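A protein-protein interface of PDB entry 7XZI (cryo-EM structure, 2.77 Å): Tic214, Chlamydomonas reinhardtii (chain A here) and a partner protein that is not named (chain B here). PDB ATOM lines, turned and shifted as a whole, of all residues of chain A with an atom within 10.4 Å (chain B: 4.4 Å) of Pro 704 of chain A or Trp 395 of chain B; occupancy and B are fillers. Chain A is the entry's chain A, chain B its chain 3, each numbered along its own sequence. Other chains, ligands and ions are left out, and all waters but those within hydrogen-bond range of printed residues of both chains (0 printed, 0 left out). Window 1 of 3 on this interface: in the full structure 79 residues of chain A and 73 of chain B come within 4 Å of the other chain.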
ATOM      1  N   ARG A 695      13.314  -8.539  10.677  1.00  0.00           N
ATOM      2  CA  ARG A 695      13.621  -9.822  11.301  1.00  0.00           C
ATOM      3  C   ARG A 695      13.954  -9.653  12.778  1.00  0.00           C
ATOM      4  O   ARG A 695      13.602 -10.510  13.597  1.00  0.00           O
ATOM      5  CB  ARG A 695      14.774 -10.513  10.573  1.00  0.00           C
ATOM      6  CG  ARG A 695      15.136 -11.858  11.178  1.00  0.00           C
ATOM      7  CD  ARG A 695      16.230 -12.565  10.405  1.00  0.00           C
ATOM      8  NE  ARG A 695      16.674 -13.762  11.103  1.00  0.00           N
ATOM      9  CZ  ARG A 695      16.119 -14.962  10.967  1.00  0.00           C
ATOM     10  NH1 ARG A 695      15.099 -15.163  10.151  1.00  0.00           N
ATOM     11  NH2 ARG A 695      16.602 -15.982  11.670  1.00  0.00           N
ATOM     12  N   ARG A 698      10.781  -9.231  14.728  1.00  0.00           N
ATOM     13  CA  ARG A 698      10.026 -10.474  14.890  1.00  0.00           C
ATOM     14  C   ARG A 698      10.025 -10.989  16.330  1.00  0.00           C
ATOM     15  O   ARG A 698       9.137 -11.765  16.701  1.00  0.00           O
ATOM     16  CB  ARG A 698      10.599 -11.540  13.946  1.00  0.00           C
ATOM     17  CG  ARG A 698       9.918 -12.901  14.002  1.00  0.00           C
ATOM     18  CD  ARG A 698      10.615 -13.900  13.093  1.00  0.00           C
ATOM     19  NE  ARG A 698      12.032 -14.031  13.403  1.00  0.00           N
ATOM     20  CZ  ARG A 698      12.544 -14.951  14.214  1.00  0.00           C
ATOM     21  NH1 ARG A 698      11.778 -15.842  14.821  1.00  0.00           N
ATOM     22  NH2 ARG A 698      13.858 -14.978  14.417  1.00  0.00           N
ATOM     23  N   TYR A 699      10.968 -10.542  17.166  1.00  0.00           N
ATOM     24  CA  TYR A 699      11.144 -11.087  18.509  1.00  0.00           C
ATOM     25  C   TYR A 699      10.021 -10.734  19.478  1.00  0.00           C
ATOM     26  O   TYR A 699       9.910 -11.386  20.521  1.00  0.00           O
ATOM     27  CB  TYR A 699      12.465 -10.596  19.104  1.00  0.00           C
ATOM     28  CG  TYR A 699      13.619 -11.554  18.938  1.00  0.00           C
ATOM     29  CD1 TYR A 699      13.721 -12.689  19.729  1.00  0.00           C
ATOM     30  CD2 TYR A 699      14.617 -11.314  18.005  1.00  0.00           C
ATOM     31  CE1 TYR A 699      14.776 -13.565  19.587  1.00  0.00           C
ATOM     32  CE2 TYR A 699      15.677 -12.184  17.856  1.00  0.00           C
ATOM     33  CZ  TYR A 699      15.752 -13.308  18.649  1.00  0.00           C
ATOM     34  OH  TYR A 699      16.805 -14.179  18.505  1.00  0.00           O
ATOM     35  N   TYR A 700       9.191  -9.738  19.177  1.00  0.00           N
ATOM     36  CA  TYR A 700       8.238  -9.219  20.150  1.00  0.00           C
ATOM     37  C   TYR A 700       6.869  -9.882  20.078  1.00  0.00           C
ATOM     38  O   TYR A 700       5.954  -9.453  20.787  1.00  0.00           O
ATOM     39  CB  TYR A 700       8.084  -7.703  19.985  1.00  0.00           C
ATOM     40  CG  TYR A 700       9.325  -6.920  20.351  1.00  0.00           C
ATOM     41  CD1 TYR A 700       9.532  -6.477  21.650  1.00  0.00           C
ATOM     42  CD2 TYR A 700      10.289  -6.628  19.399  1.00  0.00           C
ATOM     43  CE1 TYR A 700      10.664  -5.762  21.988  1.00  0.00           C
ATOM     44  CE2 TYR A 700      11.423  -5.915  19.729  1.00  0.00           C
ATOM     45  CZ  TYR A 700      11.606  -5.485  21.023  1.00  0.00           C
ATOM     46  OH  TYR A 700      12.736  -4.775  21.351  1.00  0.00           O
ATOM     47  N   GLY A 701       6.702 -10.909  19.251  1.00  0.00           N
ATOM     48  CA  GLY A 701       5.441 -11.603  19.127  1.00  0.00           C
ATOM     49  C   GLY A 701       5.631 -13.106  19.206  1.00  0.00           C
ATOM     50  O   GLY A 701       6.579 -13.609  19.811  1.00  0.00           O
ATOM     51  N   THR A 702       4.699 -13.824  18.584  1.00  0.00           N
ATOM     52  CA  THR A 702       4.799 -15.274  18.515  1.00  0.00           C
ATOM     53  C   THR A 702       5.936 -15.673  17.583  1.00  0.00           C
ATOM     54  O   THR A 702       6.057 -15.157  16.470  1.00  0.00           O
ATOM     55  CB  THR A 702       3.483 -15.876  18.024  1.00  0.00           C
ATOM     56  OG1 THR A 702       3.376 -15.696  16.608  1.00  0.00           O
ATOM     57  CG2 THR A 702       2.305 -15.186  18.692  1.00  0.00           C
ATOM     58  N   MET A 703       6.775 -16.598  18.044  1.00  0.00           N
ATOM     59  CA  MET A 703       7.912 -17.052  17.259  1.00  0.00           C
ATOM     60  C   MET A 703       8.212 -18.499  17.610  1.00  0.00           C
ATOM     61  O   MET A 703       8.042 -18.903  18.767  1.00  0.00           O
ATOM     62  CB  MET A 703       9.157 -16.185  17.506  1.00  0.00           C
ATOM     63  CG  MET A 703       9.607 -16.138  18.957  1.00  0.00           C
ATOM     64  SD  MET A 703      11.185 -15.297  19.175  1.00  0.00           S
ATOM     65  CE  MET A 703      12.252 -16.316  18.161  1.00  0.00           C
ATOM     66  N   PRO A 704       8.644 -19.303  16.641  1.00  0.00           N
ATOM     67  CA  PRO A 704       9.043 -20.679  16.947  1.00  0.00           C
ATOM     68  C   PRO A 704      10.468 -20.742  17.474  1.00  0.00           C
ATOM     69  O   PRO A 704      11.342 -19.979  17.058  1.00  0.00           O
ATOM     70  CB  PRO A 704       8.920 -21.386  15.592  1.00  0.00           C
ATOM     71  CG  PRO A 704       9.189 -20.308  14.599  1.00  0.00           C
ATOM     72  CD  PRO A 704       8.653 -19.030  15.193  1.00  0.00           C
ATOM     73  N   MET A 705      10.694 -21.669  18.405  1.00  0.00           N
ATOM     74  CA  MET A 705      12.009 -21.902  19.007  1.00  0.00           C
ATOM     75  C   MET A 705      12.319 -23.385  18.834  1.00  0.00           C
ATOM     76  O   MET A 705      12.033 -24.194  19.720  1.00  0.00           O
ATOM     77  CB  MET A 705      12.028 -21.479  20.470  1.00  0.00           C
ATOM     78  CG  MET A 705      11.585 -20.044  20.702  1.00  0.00           C
ATOM     79  SD  MET A 705      11.341 -19.659  22.445  1.00  0.00           S
ATOM     80  CE  MET A 705      10.807 -17.952  22.337  1.00  0.00           C
ATOM     81  N   ARG A 706      12.913 -23.737  17.693  1.00  0.00           N
ATOM     82  CA  ARG A 706      13.091 -25.128  17.299  1.00  0.00           C
ATOM     83  C   ARG A 706      14.540 -25.593  17.391  1.00  0.00           C
ATOM     84  O   ARG A 706      14.879 -26.653  16.856  1.00  0.00           O
ATOM     85  CB  ARG A 706      12.559 -25.344  15.882  1.00  0.00           C
ATOM     86  CG  ARG A 706      11.114 -24.923  15.689  1.00  0.00           C
ATOM     87  CD  ARG A 706      10.333 -26.001  14.967  1.00  0.00           C
ATOM     88  NE  ARG A 706      10.973 -26.385  13.718  1.00  0.00           N
ATOM     89  CZ  ARG A 706      10.628 -27.442  12.992  1.00  0.00           C
ATOM     90  NH1 ARG A 706       9.650 -28.249  13.368  1.00  0.00           N
ATOM     91  NH2 ARG A 706      11.284 -27.696  11.865  1.00  0.00           N
ATOM     92  N   LYS A 707      15.404 -24.828  18.053  1.00  0.00           N
ATOM     93  CA  LYS A 707      16.816 -25.182  18.182  1.00  0.00           C
ATOM     94  C   LYS A 707      17.215 -25.089  19.648  1.00  0.00           C
ATOM     95  O   LYS A 707      17.261 -23.992  20.214  1.00  0.00           O
ATOM     96  CB  LYS A 707      17.695 -24.280  17.317  1.00  0.00           C
ATOM     97  CG  LYS A 707      19.096 -24.826  17.092  1.00  0.00           C
ATOM     98  CD  LYS A 707      19.820 -24.063  15.997  1.00  0.00           C
ATOM     99  CE  LYS A 707      21.152 -24.710  15.653  1.00  0.00           C
ATOM    100  NZ  LYS A 707      22.118 -24.656  16.783  1.00  0.00           N
ATOM    101  N   LEU A 708      17.506 -26.235  20.257  1.00  0.00           N
ATOM    102  CA  LEU A 708      17.939 -26.295  21.646  1.00  0.00           C
ATOM    103  C   LEU A 708      19.458 -26.191  21.702  1.00  0.00           C
ATOM    104  O   LEU A 708      20.165 -27.075  21.205  1.00  0.00           O
ATOM    105  CB  LEU A 708      17.461 -27.588  22.304  1.00  0.00           C
ATOM    106  CG  LEU A 708      15.955 -27.711  22.537  1.00  0.00           C
ATOM    107  CD1 LEU A 708      15.580 -29.126  22.938  1.00  0.00           C
ATOM    108  CD2 LEU A 708      15.516 -26.722  23.600  1.00  0.00           C
ATOM    109  N   ASN A 712      20.792 -21.080  26.099  1.00  0.00           N
ATOM    110  CA  ASN A 712      19.594 -20.413  25.605  1.00  0.00           C
ATOM    111  C   ASN A 712      18.412 -20.802  26.486  1.00  0.00           C
ATOM    112  O   ASN A 712      18.062 -21.983  26.574  1.00  0.00           O
ATOM    113  CB  ASN A 712      19.330 -20.783  24.146  1.00  0.00           C
ATOM    114  CG  ASN A 712      18.180 -19.999  23.545  1.00  0.00           C
ATOM    115  OD1 ASN A 712      17.786 -18.956  24.065  1.00  0.00           O
ATOM    116  ND2 ASN A 712      17.637 -20.499  22.442  1.00  0.00           N
ATOM    117  N   ALA A 714      15.313 -19.305  26.136  1.00  0.00           N
ATOM    118  CA  ALA A 714      14.046 -19.000  25.474  1.00  0.00           C
ATOM    119  C   ALA A 714      13.100 -20.194  25.407  1.00  0.00           C
ATOM    120  O   ALA A 714      11.906 -20.021  25.708  1.00  0.00           O
ATOM    121  CB  ALA A 714      14.321 -18.423  24.081  1.00  0.00           C
ATOM    122  N   PRO A 715      13.530 -21.402  25.009  1.00  0.00           N
ATOM    123  CA  PRO A 715      12.584 -22.530  25.010  1.00  0.00           C
ATOM    124  C   PRO A 715      12.024 -22.851  26.383  1.00  0.00           C
ATOM    125  O   PRO A 715      10.860 -23.254  26.483  1.00  0.00           O
ATOM    126  CB  PRO A 715      13.419 -23.691  24.450  1.00  0.00           C
ATOM    127  CG  PRO A 715      14.827 -23.294  24.678  1.00  0.00           C
ATOM    128  CD  PRO A 715      14.850 -21.815  24.502  1.00  0.00           C
ATOM    129  N   LYS A 718       9.283 -20.355  26.942  1.00  0.00           N
ATOM    130  CA  LYS A 718       8.123 -20.705  26.126  1.00  0.00           C
ATOM    131  C   LYS A 718       7.365 -21.882  26.727  1.00  0.00           C
ATOM    132  O   LYS A 718       6.130 -21.882  26.775  1.00  0.00           O
ATOM    133  CB  LYS A 718       8.563 -21.017  24.696  1.00  0.00           C
ATOM    134  CG  LYS A 718       7.419 -21.399  23.770  1.00  0.00           C
ATOM    135  CD  LYS A 718       7.903 -21.640  22.349  1.00  0.00           C
ATOM    136  CE  LYS A 718       6.750 -22.003  21.427  1.00  0.00           C
ATOM    137  NZ  LYS A 718       6.092 -23.278  21.827  1.00  0.00           N
ATOM    138  N   ALA A 719       8.093 -22.899  27.194  1.00  0.00           N
ATOM    139  CA  ALA A 719       7.451 -24.060  27.804  1.00  0.00           C
ATOM    140  C   ALA A 719       6.712 -23.679  29.079  1.00  0.00           C
ATOM    141  O   ALA A 719       5.596 -24.152  29.322  1.00  0.00           O
ATOM    142  CB  ALA A 719       8.490 -25.144  28.089  1.00  0.00           C
ATOM    143  N   LYS A 722       3.533 -21.830  28.050  1.00  0.00           N
ATOM    144  CA  LYS A 722       2.520 -22.727  27.502  1.00  0.00           C
ATOM    145  C   LYS A 722       1.863 -23.549  28.604  1.00  0.00           C
ATOM    146  O   LYS A 722       0.632 -23.627  28.683  1.00  0.00           O
ATOM    147  CB  LYS A 722       3.146 -23.643  26.449  1.00  0.00           C
ATOM    148  CG  LYS A 722       3.618 -22.926  25.194  1.00  0.00           C
ATOM    149  CD  LYS A 722       2.492 -22.754  24.191  1.00  0.00           C
ATOM    150  CE  LYS A 722       2.050 -24.100  23.639  1.00  0.00           C
ATOM    151  NZ  LYS A 722       1.026 -23.971  22.565  1.00  0.00           N
ATOM    152  N   GLU A1139      -3.810 -31.097   4.926  1.00  0.00           N
ATOM    153  CA  GLU A1139      -3.768 -30.005   5.898  1.00  0.00           C
ATOM    154  C   GLU A1139      -3.410 -28.677   5.235  1.00  0.00           C
ATOM    155  O   GLU A1139      -4.033 -27.640   5.516  1.00  0.00           O
ATOM    156  CB  GLU A1139      -2.774 -30.332   7.014  1.00  0.00           C
ATOM    157  CG  GLU A1139      -3.171 -31.538   7.856  1.00  0.00           C
ATOM    158  CD  GLU A1139      -2.148 -31.880   8.923  1.00  0.00           C
ATOM    159  OE1 GLU A1139      -1.118 -31.179   9.015  1.00  0.00           O
ATOM    160  OE2 GLU A1139      -2.375 -32.853   9.672  1.00  0.00           O
ATOM    161  N   LEU A1143      -5.873 -25.320   5.086  1.00  0.00           N
ATOM    162  CA  LEU A1143      -5.592 -24.006   5.665  1.00  0.00           C
ATOM    163  C   LEU A1143      -5.382 -22.943   4.589  1.00  0.00           C
ATOM    164  O   LEU A1143      -5.803 -21.792   4.752  1.00  0.00           O
ATOM    165  CB  LEU A1143      -4.388 -24.074   6.610  1.00  0.00           C
ATOM    166  CG  LEU A1143      -2.963 -24.420   6.179  1.00  0.00           C
ATOM    167  CD1 LEU A1143      -2.225 -23.241   5.555  1.00  0.00           C
ATOM    168  CD2 LEU A1143      -2.231 -24.900   7.406  1.00  0.00           C
ATOM    169  N   PHE A1661      14.985 -33.330  10.586  1.00  0.00           N
ATOM    170  CA  PHE A1661      14.535 -34.692  10.345  1.00  0.00           C
ATOM    171  C   PHE A1661      14.768 -35.100   8.895  1.00  0.00           C
ATOM    172  O   PHE A1661      14.669 -34.288   7.971  1.00  0.00           O
ATOM    173  CB  PHE A1661      13.048 -34.837  10.684  1.00  0.00           C
ATOM    174  CG  PHE A1661      12.748 -34.825  12.159  1.00  0.00           C
ATOM    175  CD1 PHE A1661      13.738 -34.550  13.087  1.00  0.00           C
ATOM    176  CD2 PHE A1661      11.472 -35.104  12.615  1.00  0.00           C
ATOM    177  CE1 PHE A1661      13.456 -34.540  14.437  1.00  0.00           C
ATOM    178  CE2 PHE A1661      11.186 -35.099  13.965  1.00  0.00           C
ATOM    179  CZ  PHE A1661      12.180 -34.818  14.876  1.00  0.00           C
ATOM    180  N   PHE A1663      13.126 -37.630   6.267  1.00  0.00           N
ATOM    181  CA  PHE A1663      11.857 -38.341   6.111  1.00  0.00           C
ATOM    182  C   PHE A1663      12.063 -39.658   5.358  1.00  0.00           C
ATOM    183  O   PHE A1663      11.481 -39.914   4.305  1.00  0.00           O
ATOM    184  CB  PHE A1663      10.845 -37.450   5.402  1.00  0.00           C
ATOM    185  CG  PHE A1663      10.651 -36.114   6.059  1.00  0.00           C
ATOM    186  CD1 PHE A1663      10.678 -35.992   7.439  1.00  0.00           C
ATOM    187  CD2 PHE A1663      10.451 -34.974   5.296  1.00  0.00           C
ATOM    188  CE1 PHE A1663      10.504 -34.764   8.044  1.00  0.00           C
ATOM    189  CE2 PHE A1663      10.278 -33.743   5.898  1.00  0.00           C
ATOM    190  CZ  PHE A1663      10.303 -33.640   7.273  1.00  0.00           C
ATOM    191  N   ALA B 340       5.326 -24.889   6.702  1.00  0.00           N
ATOM    192  CA  ALA B 340       5.249 -25.275   8.107  1.00  0.00           C
ATOM    193  C   ALA B 340       4.143 -26.297   8.334  1.00  0.00           C
ATOM    194  O   ALA B 340       4.306 -27.243   9.120  1.00  0.00           O
ATOM    195  CB  ALA B 340       5.025 -24.039   8.977  1.00  0.00           C
ATOM    196  N   ARG B 344       5.165 -29.956   9.964  1.00  0.00           N
ATOM    197  CA  ARG B 344       4.718 -30.442  11.267  1.00  0.00           C
ATOM    198  C   ARG B 344       4.256 -31.893  11.183  1.00  0.00           C
ATOM    199  O   ARG B 344       4.665 -32.736  11.992  1.00  0.00           O
ATOM    200  CB  ARG B 344       3.596 -29.557  11.811  1.00  0.00           C
ATOM    201  CG  ARG B 344       3.014 -30.066  13.122  1.00  0.00           C
ATOM    202  CD  ARG B 344       1.716 -29.363  13.479  1.00  0.00           C
ATOM    203  NE  ARG B 344       1.034 -30.020  14.584  1.00  0.00           N
ATOM    204  CZ  ARG B 344       0.214 -31.056  14.449  1.00  0.00           C
ATOM    205  NH1 ARG B 344      -0.040 -31.586  13.264  1.00  0.00           N
ATOM    206  NH2 ARG B 344      -0.364 -31.573  15.529  1.00  0.00           N
ATOM    207  N   ARG B 386       9.853 -28.531  19.625  1.00  0.00           N
ATOM    208  CA  ARG B 386       9.491 -28.866  18.252  1.00  0.00           C
ATOM    209  C   ARG B 386       8.326 -28.020  17.752  1.00  0.00           C
ATOM    210  O   ARG B 386       8.176 -27.830  16.541  1.00  0.00           O
ATOM    211  CB  ARG B 386       9.156 -30.354  18.142  1.00  0.00           C
ATOM    212  CG  ARG B 386      10.364 -31.279  18.192  1.00  0.00           C
ATOM    213  CD  ARG B 386      11.200 -31.189  16.923  1.00  0.00           C
ATOM    214  NE  ARG B 386      12.179 -30.113  16.976  1.00  0.00           N
ATOM    215  CZ  ARG B 386      12.973 -29.769  15.967  1.00  0.00           C
ATOM    216  NH1 ARG B 386      12.924 -30.398  14.804  1.00  0.00           N
ATOM    217  NH2 ARG B 386      13.834 -28.771  16.131  1.00  0.00           N
ATOM    218  N   GLY B 387       7.494 -27.513  18.659  1.00  0.00           N
ATOM    219  CA  GLY B 387       6.395 -26.654  18.268  1.00  0.00           C
ATOM    220  C   GLY B 387       5.219 -27.361  17.642  1.00  0.00           C
ATOM    221  O   GLY B 387       4.428 -26.725  16.939  1.00  0.00           O
ATOM    222  N   ASP B 390       1.810 -26.056  19.074  1.00  0.00           N
ATOM    223  CA  ASP B 390       1.420 -24.719  18.658  1.00  0.00           C
ATOM    224  C   ASP B 390       0.707 -24.768  17.309  1.00  0.00           C
ATOM    225  O   ASP B 390       1.027 -25.616  16.468  1.00  0.00           O
ATOM    226  CB  ASP B 390       2.647 -23.810  18.563  1.00  0.00           C
ATOM    227  CG  ASP B 390       3.428 -23.751  19.858  1.00  0.00           C
ATOM    228  OD1 ASP B 390       3.991 -24.790  20.263  1.00  0.00           O
ATOM    229  OD2 ASP B 390       3.483 -22.664  20.469  1.00  0.00           O
ATOM    230  N   PRO B 391      -0.262 -23.887  17.072  1.00  0.00           N
ATOM    231  CA  PRO B 391      -0.867 -23.797  15.739  1.00  0.00           C
ATOM    232  C   PRO B 391       0.147 -23.325  14.711  1.00  0.00           C
ATOM    233  O   PRO B 391       1.123 -22.644  15.033  1.00  0.00           O
ATOM    234  CB  PRO B 391      -1.995 -22.775  15.927  1.00  0.00           C
ATOM    235  CG  PRO B 391      -1.597 -21.988  17.134  1.00  0.00           C
ATOM    236  CD  PRO B 391      -0.884 -22.955  18.027  1.00  0.00           C
ATOM    237  N   VAL B 392      -0.093 -23.708  13.454  1.00  0.00           N
ATOM    238  CA  VAL B 392       0.874 -23.428  12.396  1.00  0.00           C
ATOM    239  C   VAL B 392       1.072 -21.930  12.205  1.00  0.00           C
ATOM    240  O   VAL B 392       2.159 -21.488  11.811  1.00  0.00           O
ATOM    241  CB  VAL B 392       0.443 -24.112  11.085  1.00  0.00           C
ATOM    242  CG1 VAL B 392       0.608 -25.616  11.198  1.00  0.00           C
ATOM    243  CG2 VAL B 392      -0.995 -23.756  10.750  1.00  0.00           C
ATOM    244  N   GLN B 393       0.047 -21.125  12.496  1.00  0.00           N
ATOM    245  CA  GLN B 393       0.173 -19.680  12.329  1.00  0.00           C
ATOM    246  C   GLN B 393       1.283 -19.109  13.203  1.00  0.00           C
ATOM    247  O   GLN B 393       2.066 -18.270  12.741  1.00  0.00           O
ATOM    248  CB  GLN B 393      -1.156 -18.990  12.643  1.00  0.00           C
ATOM    249  CG  GLN B 393      -2.264 -19.256  11.632  1.00  0.00           C
ATOM    250  CD  GLN B 393      -2.936 -20.599  11.834  1.00  0.00           C
ATOM    251  OE1 GLN B 393      -2.633 -21.322  12.782  1.00  0.00           O
ATOM    252  NE2 GLN B 393      -3.857 -20.940  10.939  1.00  0.00           N
ATOM    253  N   ASN B 394       1.391 -19.571  14.450  1.00  0.00           N
ATOM    254  CA  ASN B 394       2.460 -19.111  15.328  1.00  0.00           C
ATOM    255  C   ASN B 394       3.842 -19.425  14.771  1.00  0.00           C
ATOM    256  O   ASN B 394       4.822 -18.806  15.198  1.00  0.00           O
ATOM    257  CB  ASN B 394       2.315 -19.735  16.717  1.00  0.00           C
ATOM    258  CG  ASN B 394       0.995 -19.392  17.376  1.00  0.00           C
ATOM    259  OD1 ASN B 394       0.046 -18.971  16.714  1.00  0.00           O
ATOM    260  ND2 ASN B 394       0.927 -19.576  18.688  1.00  0.00           N
ATOM    261  N   TRP B 395       3.940 -20.377  13.841  1.00  0.00           N
ATOM    262  CA  TRP B 395       5.216 -20.645  13.189  1.00  0.00           C
ATOM    263  C   TRP B 395       5.663 -19.456  12.348  1.00  0.00           C
ATOM    264  O   TRP B 395       6.846 -19.096  12.345  1.00  0.00           O
ATOM    265  CB  TRP B 395       5.119 -21.907  12.329  1.00  0.00           C
ATOM    266  CG  TRP B 395       5.009 -23.178  13.117  1.00  0.00           C
ATOM    267  CD1 TRP B 395       4.237 -23.398  14.221  1.00  0.00           C
ATOM    268  CD2 TRP B 395       5.707 -24.405  12.867  1.00  0.00           C
ATOM    269  NE1 TRP B 395       4.406 -24.686  14.668  1.00  0.00           N
ATOM    270  CE2 TRP B 395       5.304 -25.324  13.855  1.00  0.00           C
ATOM    271  CE3 TRP B 395       6.634 -24.814  11.904  1.00  0.00           C
ATOM    272  CZ2 TRP B 395       5.793 -26.627  13.907  1.00  0.00           C
ATOM    273  CZ3 TRP B 395       7.116 -26.107  11.955  1.00  0.00           C
ATOM    274  CH2 TRP B 395       6.696 -26.998  12.949  1.00  0.00           C
ATOM    275  N   VAL B 396       4.732 -18.829  11.623  1.00  0.00           N
ATOM    276  CA  VAL B 396       5.135 -17.773  10.699  1.00  0.00           C
ATOM    277  C   VAL B 396       5.263 -16.438  11.423  1.00  0.00           C
ATOM    278  O   VAL B 396       6.016 -15.555  10.993  1.00  0.00           O
ATOM    279  CB  VAL B 396       4.170 -17.690   9.503  1.00  0.00           C
ATOM    280  CG1 VAL B 396       4.112 -19.027   8.776  1.00  0.00           C
ATOM    281  CG2 VAL B 396       2.788 -17.247   9.946  1.00  0.00           C
ATOM    282  N   GLY B 397       4.537 -16.260  12.524  1.00  0.00           N
ATOM    283  CA  GLY B 397       4.707 -15.063  13.324  1.00  0.00           C
ATOM    284  C   GLY B 397       3.421 -14.426  13.806  1.00  0.00           C
ATOM    285  O   GLY B 397       3.441 -13.604  14.726  1.00  0.00           O
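Among the printed residues, pairs that only touch across the chains: Arg 706 of chain A with Trp 395 of chain B (3.2 Å), Pro 704 of chain A with Trp 395 of chain B (3.4 Å), Thr 702 of chain A with Asn 394 of chain B (3.7 Å), Leu 1143 of chain A with Val 392 of chain B (3.7 Å) and Pro 704 of chain A with Asn 394 of chain B (3.8 Å).
NH2 of Arg 386 of chain B lies within hydrogen-bond range of O of Arg 706 of chain A (2.5 Å).
The side-chain amino group of Lys 722 of chain A is in salt-bridge range of the side-chain carboxylate of Asp 390 of chain B (3.5 Å).
OD2 of Asp 390 of chain B lies within salt-bridge range of NZ of Lys 718 of chain A (3.0 Å).
O of Gly 397 of chain B lies within hydrogen-bond range of OG1 of Thr 702 of chain A (2.8 Å).
O of Gly 387 of chain B lies within hydrogen-bond range of NE1 of Trp 395 of chain B.
Printed residues of chain B that touch a printed residue of chain A: Arg 386, Asp 390, Val 392, Asn 394, Trp 395 and Gly 397.
Hydrophobic or aromatic side chains of chain A that line the printed part of chain B: Pro 704 and Leu 1143.
Along chain A the printed residues that touch a printed residue of chain B span positions 702 to 1143.
Of chain B, only Asn 394 and Trp 395 come within 4 Å of Pro 704 of chain A.
Trp 395 of chain B touches two residues of chain A.
No residue of chain A comes within 4 Å of Ala 340 of chain B.
No residue of chain A comes within 4 Å of Gly 387 of chain B.
Val 392 of chain B touches just one residue of chain A: Leu 1143.
Of chain A, only Thr 702 and Pro 704 come within 4 Å of Asn 394 of chain B.
No residue of chain A comes within 4 Å of Val 396 of chain B.
Printed residues of chain B within 4 Å of Lys 718 of chain A: Asp 390 (3.0 Å).
Printed residues of chain B within 4 Å of Arg 706 of chain A: Arg 386 and Trp 395.
Tyr 700 of chain A touches none of the printed residues of chain B.
Met 703 of chain A touches none of the printed residues of chain B.
The nearest printed residue of chain B that does not touch Pro 704 of chain A is Val 396 of chain B (5.3 Å).
The nearest residue of chain A that does not touch Trp 395 of chain B is Met 703 of chain A (5.4 Å).
The nearest printed residue of chain B that does not touch Lys 722 of chain A is Pro 391 of chain B (5.0 Å).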
